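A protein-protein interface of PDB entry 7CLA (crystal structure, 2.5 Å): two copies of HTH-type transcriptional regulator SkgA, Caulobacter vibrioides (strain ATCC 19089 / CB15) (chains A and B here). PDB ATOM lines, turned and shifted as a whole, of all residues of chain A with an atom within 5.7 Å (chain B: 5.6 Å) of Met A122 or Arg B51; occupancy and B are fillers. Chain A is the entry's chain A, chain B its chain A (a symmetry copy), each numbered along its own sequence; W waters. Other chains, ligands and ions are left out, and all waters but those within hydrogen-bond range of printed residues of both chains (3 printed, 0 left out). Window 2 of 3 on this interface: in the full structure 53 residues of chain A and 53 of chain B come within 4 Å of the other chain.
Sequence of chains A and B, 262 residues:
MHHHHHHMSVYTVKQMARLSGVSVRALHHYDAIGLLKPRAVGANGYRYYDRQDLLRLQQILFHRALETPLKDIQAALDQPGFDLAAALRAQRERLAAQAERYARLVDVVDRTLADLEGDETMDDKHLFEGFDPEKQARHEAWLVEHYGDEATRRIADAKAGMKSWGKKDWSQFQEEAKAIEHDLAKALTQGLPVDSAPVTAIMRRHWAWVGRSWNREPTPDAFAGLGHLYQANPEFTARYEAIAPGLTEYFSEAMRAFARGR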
ATOM      1  N   ARG A 111      22.325 -21.238 -34.098  1.00  0.00           N
ATOM      2  CA  ARG A 111      21.569 -22.286 -33.415  1.00  0.00           C
ATOM      3  C   ARG A 111      20.344 -21.670 -32.728  1.00  0.00           C
ATOM      4  O   ARG A 111      19.254 -22.321 -32.714  1.00  0.00           O
ATOM      5  CB  ARG A 111      22.496 -22.913 -32.405  1.00  0.00           C
ATOM      6  CG  ARG A 111      22.088 -24.305 -32.026  1.00  0.00           C
ATOM      7  CD  ARG A 111      23.088 -24.863 -31.047  1.00  0.00           C
ATOM      8  NE  ARG A 111      22.683 -26.253 -30.814  1.00  0.00           N
ATOM      9  CZ  ARG A 111      23.380 -27.091 -30.087  1.00  0.00           C
ATOM     10  NH1 ARG A 111      24.510 -26.676 -29.535  1.00  0.00           N
ATOM     11  NH2 ARG A 111      22.987 -28.336 -29.959  1.00  0.00           N
ATOM     12  N   THR A 112      20.517 -20.476 -32.165  1.00  0.00           N
ATOM     13  CA  THR A 112      19.495 -19.739 -31.391  1.00  0.00           C
ATOM     14  C   THR A 112      18.413 -19.255 -32.362  1.00  0.00           C
ATOM     15  O   THR A 112      17.264 -19.403 -32.046  1.00  0.00           O
ATOM     16  CB  THR A 112      20.160 -18.594 -30.607  1.00  0.00           C
ATOM     17  OG1 THR A 112      21.183 -19.196 -29.816  1.00  0.00           O
ATOM     18  CG2 THR A 112      19.188 -17.770 -29.772  1.00  0.00           C
ATOM     19  N   ASP A 115      16.267 -22.288 -33.526  1.00  0.00           N
ATOM     20  CA  ASP A 115      15.370 -22.715 -32.434  1.00  0.00           C
ATOM     21  C   ASP A 115      14.195 -21.745 -32.387  1.00  0.00           C
ATOM     22  O   ASP A 115      13.028 -22.165 -32.343  1.00  0.00           O
ATOM     23  CB  ASP A 115      16.077 -22.706 -31.069  1.00  0.00           C
ATOM     24  CG  ASP A 115      15.274 -23.403 -29.967  1.00  0.00           C
ATOM     25  OD1 ASP A 115      14.967 -24.619 -30.123  1.00  0.00           O
ATOM     26  OD2 ASP A 115      14.949 -22.759 -29.008  1.00  0.00           O
ATOM     27  N   GLU A 120      11.156 -24.119 -30.583  1.00  0.00           N
ATOM     28  CA  GLU A 120      11.770 -23.581 -29.343  1.00  0.00           C
ATOM     29  C   GLU A 120      12.000 -24.698 -28.324  1.00  0.00           C
ATOM     30  O   GLU A 120      11.878 -24.435 -27.108  1.00  0.00           O
ATOM     31  CB  GLU A 120      10.922 -22.436 -28.799  1.00  0.00           C
ATOM     32  CG  GLU A 120      10.625 -21.352 -29.828  1.00  0.00           C
ATOM     33  CD  GLU A 120      10.251 -20.013 -29.192  1.00  0.00           C
ATOM     34  OE1 GLU A 120       9.708 -20.013 -28.074  1.00  0.00           O
ATOM     35  OE2 GLU A 120      10.536 -18.960 -29.779  1.00  0.00           O
ATOM     36  N   THR A 121      12.451 -25.854 -28.799  1.00  0.00           N
ATOM     37  CA  THR A 121      12.740 -27.049 -27.959  1.00  0.00           C
ATOM     38  C   THR A 121      14.241 -27.110 -27.569  1.00  0.00           C
ATOM     39  O   THR A 121      14.624 -27.918 -26.702  1.00  0.00           O
ATOM     40  CB  THR A 121      12.254 -28.305 -28.705  1.00  0.00           C
ATOM     41  OG1 THR A 121      12.964 -28.361 -29.952  1.00  0.00           O
ATOM     42  CG2 THR A 121      10.756 -28.294 -28.971  1.00  0.00           C
ATOM     43  N   MET A 122      15.126 -26.326 -28.192  1.00  0.00           N
ATOM     44  CA  MET A 122      16.587 -26.410 -27.881  1.00  0.00           C
ATOM     45  C   MET A 122      16.783 -26.214 -26.357  1.00  0.00           C
ATOM     46  O   MET A 122      16.172 -25.326 -25.745  1.00  0.00           O
ATOM     47  CB  MET A 122      17.418 -25.404 -28.703  1.00  0.00           C
ATOM     48  CG  MET A 122      18.828 -25.247 -28.282  1.00  0.00           C
ATOM     49  SD  MET A 122      19.719 -24.095 -29.284  1.00  0.00           S
ATOM     50  CE  MET A 122      19.533 -22.589 -28.351  1.00  0.00           C
ATOM     51  N   ASP A 123      17.594 -27.071 -25.766  1.00  0.00           N
ATOM     52  CA  ASP A 123      18.010 -26.978 -24.351  1.00  0.00           C
ATOM     53  C   ASP A 123      18.573 -25.566 -24.075  1.00  0.00           C
ATOM     54  O   ASP A 123      19.408 -25.035 -24.836  1.00  0.00           O
ATOM     55  CB  ASP A 123      19.020 -28.085 -24.029  1.00  0.00           C
ATOM     56  CG  ASP A 123      19.063 -28.488 -22.561  1.00  0.00           C
ATOM     57  OD1 ASP A 123      19.595 -27.656 -21.634  1.00  0.00           O
ATOM     58  OD2 ASP A 123      18.594 -29.625 -22.326  1.00  0.00           O
ATOM     59  N   ASP A 124      18.161 -24.987 -22.963  1.00  0.00           N
ATOM     60  CA  ASP A 124      18.653 -23.704 -22.413  1.00  0.00           C
ATOM     61  C   ASP A 124      20.183 -23.602 -22.350  1.00  0.00           C
ATOM     62  O   ASP A 124      20.688 -22.454 -22.451  1.00  0.00           O
ATOM     63  CB  ASP A 124      18.092 -23.513 -21.011  1.00  0.00           C
ATOM     64  CG  ASP A 124      16.633 -23.161 -21.007  1.00  0.00           C
ATOM     65  OD1 ASP A 124      16.082 -22.791 -22.101  1.00  0.00           O
ATOM     66  OD2 ASP A 124      16.057 -23.234 -19.912  1.00  0.00           O
ATOM     67  N   HIS A 126      22.460 -24.393 -24.220  1.00  0.00           N
ATOM     68  CA  HIS A 126      23.106 -24.156 -25.535  1.00  0.00           C
ATOM     69  C   HIS A 126      23.143 -22.664 -25.868  1.00  0.00           C
ATOM     70  O   HIS A 126      23.974 -22.292 -26.722  1.00  0.00           O
ATOM     71  CB  HIS A 126      22.452 -24.968 -26.626  1.00  0.00           C
ATOM     72  CG  HIS A 126      22.697 -26.437 -26.436  1.00  0.00           C
ATOM     73  ND1 HIS A 126      23.974 -26.958 -26.355  1.00  0.00           N
ATOM     74  CD2 HIS A 126      21.831 -27.479 -26.267  1.00  0.00           C
ATOM     75  CE1 HIS A 126      23.876 -28.271 -26.175  1.00  0.00           C
ATOM     76  NE2 HIS A 126      22.565 -28.605 -26.111  1.00  0.00           N
ATOM     77  N   LEU A 127      22.332 -21.858 -25.180  1.00  0.00           N
ATOM     78  CA  LEU A 127      22.313 -20.389 -25.322  1.00  0.00           C
ATOM     79  C   LEU A 127      23.656 -19.807 -24.888  1.00  0.00           C
ATOM     80  O   LEU A 127      23.991 -18.700 -25.387  1.00  0.00           O
ATOM     81  CB  LEU A 127      21.189 -19.799 -24.466  1.00  0.00           C
ATOM     82  CG  LEU A 127      19.785 -20.166 -24.938  1.00  0.00           C
ATOM     83  CD1 LEU A 127      18.728 -19.717 -23.923  1.00  0.00           C
ATOM     84  CD2 LEU A 127      19.511 -19.606 -26.350  1.00  0.00           C
ATOM     85  N   HIS B   7      12.691 -23.659 -22.047  1.00  0.00           N
ATOM     86  CA  HIS B   7      11.276 -23.362 -22.482  1.00  0.00           C
ATOM     87  C   HIS B   7      10.413 -23.008 -21.260  1.00  0.00           C
ATOM     88  O   HIS B   7      10.191 -21.813 -21.025  1.00  0.00           O
ATOM     89  CB  HIS B   7      10.628 -24.527 -23.253  1.00  0.00           C
ATOM     90  CG  HIS B   7       9.437 -24.083 -24.049  1.00  0.00           C
ATOM     91  ND1 HIS B   7       8.578 -23.040 -23.626  1.00  0.00           N
ATOM     92  CD2 HIS B   7       8.970 -24.495 -25.253  1.00  0.00           C
ATOM     93  CE1 HIS B   7       7.640 -22.836 -24.546  1.00  0.00           C
ATOM     94  NE2 HIS B   7       7.857 -23.725 -25.556  1.00  0.00           N
ATOM     95  N   SER B   9      11.162 -24.212 -18.163  1.00  0.00           N
ATOM     96  CA  SER B   9      12.157 -24.195 -17.061  1.00  0.00           C
ATOM     97  C   SER B   9      12.353 -22.776 -16.520  1.00  0.00           C
ATOM     98  O   SER B   9      12.366 -21.828 -17.309  1.00  0.00           O
ATOM     99  CB  SER B   9      13.447 -24.754 -17.472  1.00  0.00           C
ATOM    100  OG  SER B   9      13.250 -25.937 -18.230  1.00  0.00           O
ATOM    101  N   TYR B  49      14.261 -16.657 -13.180  1.00  0.00           N
ATOM    102  CA  TYR B  49      14.573 -16.322 -14.569  1.00  0.00           C
ATOM    103  C   TYR B  49      13.853 -17.338 -15.434  1.00  0.00           C
ATOM    104  O   TYR B  49      14.054 -18.617 -15.254  1.00  0.00           O
ATOM    105  CB  TYR B  49      16.086 -16.333 -14.815  1.00  0.00           C
ATOM    106  CG  TYR B  49      16.853 -15.362 -13.955  1.00  0.00           C
ATOM    107  CD1 TYR B  49      17.286 -14.143 -14.466  1.00  0.00           C
ATOM    108  CD2 TYR B  49      17.246 -15.696 -12.657  1.00  0.00           C
ATOM    109  CE1 TYR B  49      18.043 -13.270 -13.699  1.00  0.00           C
ATOM    110  CE2 TYR B  49      17.986 -14.802 -11.874  1.00  0.00           C
ATOM    111  CZ  TYR B  49      18.349 -13.575 -12.384  1.00  0.00           C
ATOM    112  OH  TYR B  49      19.047 -12.705 -11.608  1.00  0.00           O
ATOM    113  N   ASP B  50      13.135 -16.819 -16.425  1.00  0.00           N
ATOM    114  CA  ASP B  50      12.470 -17.693 -17.419  1.00  0.00           C
ATOM    115  C   ASP B  50      13.214 -17.581 -18.755  1.00  0.00           C
ATOM    116  O   ASP B  50      14.165 -16.779 -18.857  1.00  0.00           O
ATOM    117  CB  ASP B  50      10.967 -17.405 -17.419  1.00  0.00           C
ATOM    118  CG  ASP B  50      10.576 -16.119 -18.123  1.00  0.00           C
ATOM    119  OD1 ASP B  50      11.471 -15.466 -18.723  1.00  0.00           O
ATOM    120  OD2 ASP B  50       9.364 -15.774 -18.046  1.00  0.00           O
ATOM    121  N   ARG B  51      12.757 -18.342 -19.750  1.00  0.00           N
ATOM    122  CA  ARG B  51      13.283 -18.348 -21.123  1.00  0.00           C
ATOM    123  C   ARG B  51      13.513 -16.930 -21.658  1.00  0.00           C
ATOM    124  O   ARG B  51      14.542 -16.708 -22.240  1.00  0.00           O
ATOM    125  CB  ARG B  51      12.329 -19.112 -22.008  1.00  0.00           C
ATOM    126  CG  ARG B  51      12.804 -19.234 -23.445  1.00  0.00           C
ATOM    127  CD  ARG B  51      14.079 -20.057 -23.552  1.00  0.00           C
ATOM    128  NE  ARG B  51      14.387 -20.388 -24.941  1.00  0.00           N
ATOM    129  CZ  ARG B  51      15.044 -21.469 -25.349  1.00  0.00           C
ATOM    130  NH1 ARG B  51      15.224 -21.646 -26.636  1.00  0.00           N
ATOM    131  NH2 ARG B  51      15.530 -22.366 -24.497  1.00  0.00           N
ATOM    132  N   GLN B  52      12.591 -16.000 -21.471  1.00  0.00           N
ATOM    133  CA  GLN B  52      12.707 -14.612 -21.980  1.00  0.00           C
ATOM    134  C   GLN B  52      13.893 -13.914 -21.302  1.00  0.00           C
ATOM    135  O   GLN B  52      14.625 -13.173 -22.032  1.00  0.00           O
ATOM    136  CB  GLN B  52      11.395 -13.832 -21.787  1.00  0.00           C
ATOM    137  CG  GLN B  52      10.219 -14.388 -22.608  1.00  0.00           C
ATOM    138  CD  GLN B  52      10.494 -14.496 -24.095  1.00  0.00           C
ATOM    139  OE1 GLN B  52      10.765 -13.502 -24.789  1.00  0.00           O
ATOM    140  NE2 GLN B  52      10.467 -15.727 -24.594  1.00  0.00           N
ATOM    141  N   ASP B  53      14.083 -14.147 -19.999  1.00  0.00           N
ATOM    142  CA  ASP B  53      15.224 -13.638 -19.203  1.00  0.00           C
ATOM    143  C   ASP B  53      16.532 -14.264 -19.742  1.00  0.00           C
ATOM    144  O   ASP B  53      17.523 -13.583 -19.806  1.00  0.00           O
ATOM    145  CB  ASP B  53      15.089 -13.983 -17.714  1.00  0.00           C
ATOM    146  CG  ASP B  53      13.901 -13.346 -17.014  1.00  0.00           C
ATOM    147  OD1 ASP B  53      13.655 -12.168 -17.318  1.00  0.00           O
ATOM    148  OD2 ASP B  53      13.190 -14.033 -16.177  1.00  0.00           O
ATOM    149  N   LEU B  54      16.520 -15.552 -20.087  1.00  0.00           N
ATOM    150  CA  LEU B  54      17.721 -16.250 -20.591  1.00  0.00           C
ATOM    151  C   LEU B  54      18.155 -15.601 -21.918  1.00  0.00           C
ATOM    152  O   LEU B  54      19.416 -15.372 -22.140  1.00  0.00           O
ATOM    153  CB  LEU B  54      17.401 -17.740 -20.733  1.00  0.00           C
ATOM    154  CG  LEU B  54      17.803 -18.568 -19.520  1.00  0.00           C
ATOM    155  CD1 LEU B  54      16.836 -18.362 -18.408  1.00  0.00           C
ATOM    156  CD2 LEU B  54      17.878 -20.035 -19.882  1.00  0.00           C
ATOM    157  N   LEU B  55      17.176 -15.289 -22.756  1.00  0.00           N
ATOM    158  CA  LEU B  55      17.417 -14.660 -24.070  1.00  0.00           C
ATOM    159  C   LEU B  55      17.942 -13.223 -23.858  1.00  0.00           C
ATOM    160  O   LEU B  55      18.846 -12.816 -24.642  1.00  0.00           O
ATOM    161  CB  LEU B  55      16.116 -14.724 -24.878  1.00  0.00           C
ATOM    162  CG  LEU B  55      15.774 -16.134 -25.365  1.00  0.00           C
ATOM    163  CD1 LEU B  55      14.364 -16.191 -25.890  1.00  0.00           C
ATOM    164  CD2 LEU B  55      16.734 -16.613 -26.432  1.00  0.00           C
ATOM    165  N   ARG B  56      17.398 -12.481 -22.881  1.00  0.00           N
ATOM    166  CA  ARG B  56      17.924 -11.140 -22.555  1.00  0.00           C
ATOM    167  C   ARG B  56      19.355 -11.299 -22.035  1.00  0.00           C
ATOM    168  O   ARG B  56      20.192 -10.530 -22.421  1.00  0.00           O
ATOM    169  CB  ARG B  56      17.017 -10.361 -21.583  1.00  0.00           C
ATOM    170  CG  ARG B  56      17.532  -8.961 -21.257  1.00  0.00           C
ATOM    171  CD  ARG B  56      16.724  -8.180 -20.214  1.00  0.00           C
ATOM    172  NE  ARG B  56      15.846  -7.304 -20.938  1.00  0.00           N
ATOM    173  CZ  ARG B  56      15.851  -5.997 -20.921  1.00  0.00           C
ATOM    174  NH1 ARG B  56      16.625  -5.327 -20.098  1.00  0.00           N
ATOM    175  NH2 ARG B  56      15.028  -5.364 -21.719  1.00  0.00           N
HETATM  176  O   HOH W   1      10.898 -16.640 -27.294  1.00  0.00           O
HETATM  177  O   HOH W   2      13.602 -21.854 -19.931  1.00  0.00           O
HETATM  178  O   HOH W   3      12.733 -19.552 -27.094  1.00  0.00           O
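The side-chain carboxylate (OD2) of Asp A115 is in salt-bridge range of the guanidinium group (NH1) of Arg B51, 2.6 Å away.
O of Met A122 sits at hydrogen-bond distance from NH2 of Arg B51 (3.3 Å).
The guanidinium group (NH2) of Arg B51 is in salt-bridge range of the side-chain carboxylate (OD1) of Asp A124 (2.5 Å).
Hydrophobic or aromatic side chains of chain A that line the printed part of chain B: Leu A127.
Hydrophobic or aromatic side chains of chain B that line the printed part of chain A: His B7 and Leu B54.
Among the printed residues, merely in contact across the chains: Glu A120 with His B7 (3.4 Å), Asp A124 with His B7 (3.5 Å), Asp A124 with Ser B9 (3.9 Å), Asp A124 with Leu B54 (3.5 Å) and Leu A127 with Leu B54 (3.98 Å).
Water W2 lies within hydrogen-bond range of the side-chain carboxylate (OD2) of Asp A124 (2.8 Å), the backbone carbonyl oxygen (O) of Ser B9 (2.9 Å) and the backbone NH (N) of His B7 (2.9 Å).
Water W3 lies within hydrogen-bond range of NE of Arg B51 and OE1 of Glu A120.
Water W1 bridges NE2 of Gln B52 (2.9 Å) and OE2 of Glu A120 (3.4 Å).
Of chain B, only Arg B51 comes within 4 Å of Met A122.
Of chain A, only Asp A115 (2.6 Å), Met A122 (3.3 Å) and Asp A124 (2.5 Å) come within 4 Å of Arg B51.
Printed residues of chain B within 4 Å of Glu A120: His B7 (3.4 Å).
Of the printed residues of chain A, Leu B54 touches Asp A124 (3.5 Å) and Leu A127 (3.98 Å).
Of the printed residues of chain B, Asp A124 touches His B7 (3.5 Å), Ser B9 (3.9 Å), Arg B51 (2.5 Å) and Leu B54 (3.5 Å).
Printed residues of chain A within 4 Å of His B7: Glu A120 (3.4 Å) and Asp A124 (3.5 Å).
Of the printed residues of chain A, Ser B9 touches Asp A124.
Arg A111 touches none of the printed residues of chain B.
Asp A123 touches none of the printed residues of chain B.
The nearest residue of chain A that does not touch Arg B51 is Leu A127 (4.2 Å).
The nearest printed residue of chain B that does not touch Asp A124 is Asp B50 (6.4 Å).
The backbone carbonyl oxygen of Asp A115 is in hydrogen-bond range of the backbone NH of Glu A120 (3.2 Å).
The side-chain carboxylate (OD1) of Asp A115 lies within hydrogen-bond range of the backbone NH (N) of Thr A121 (3.1 Å).
The side-chain carboxylate (OD1) of Asp A115 is in hydrogen-bond range of the backbone NH (N) of Met A122 (2.6 Å).
No position is printed for both chains.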
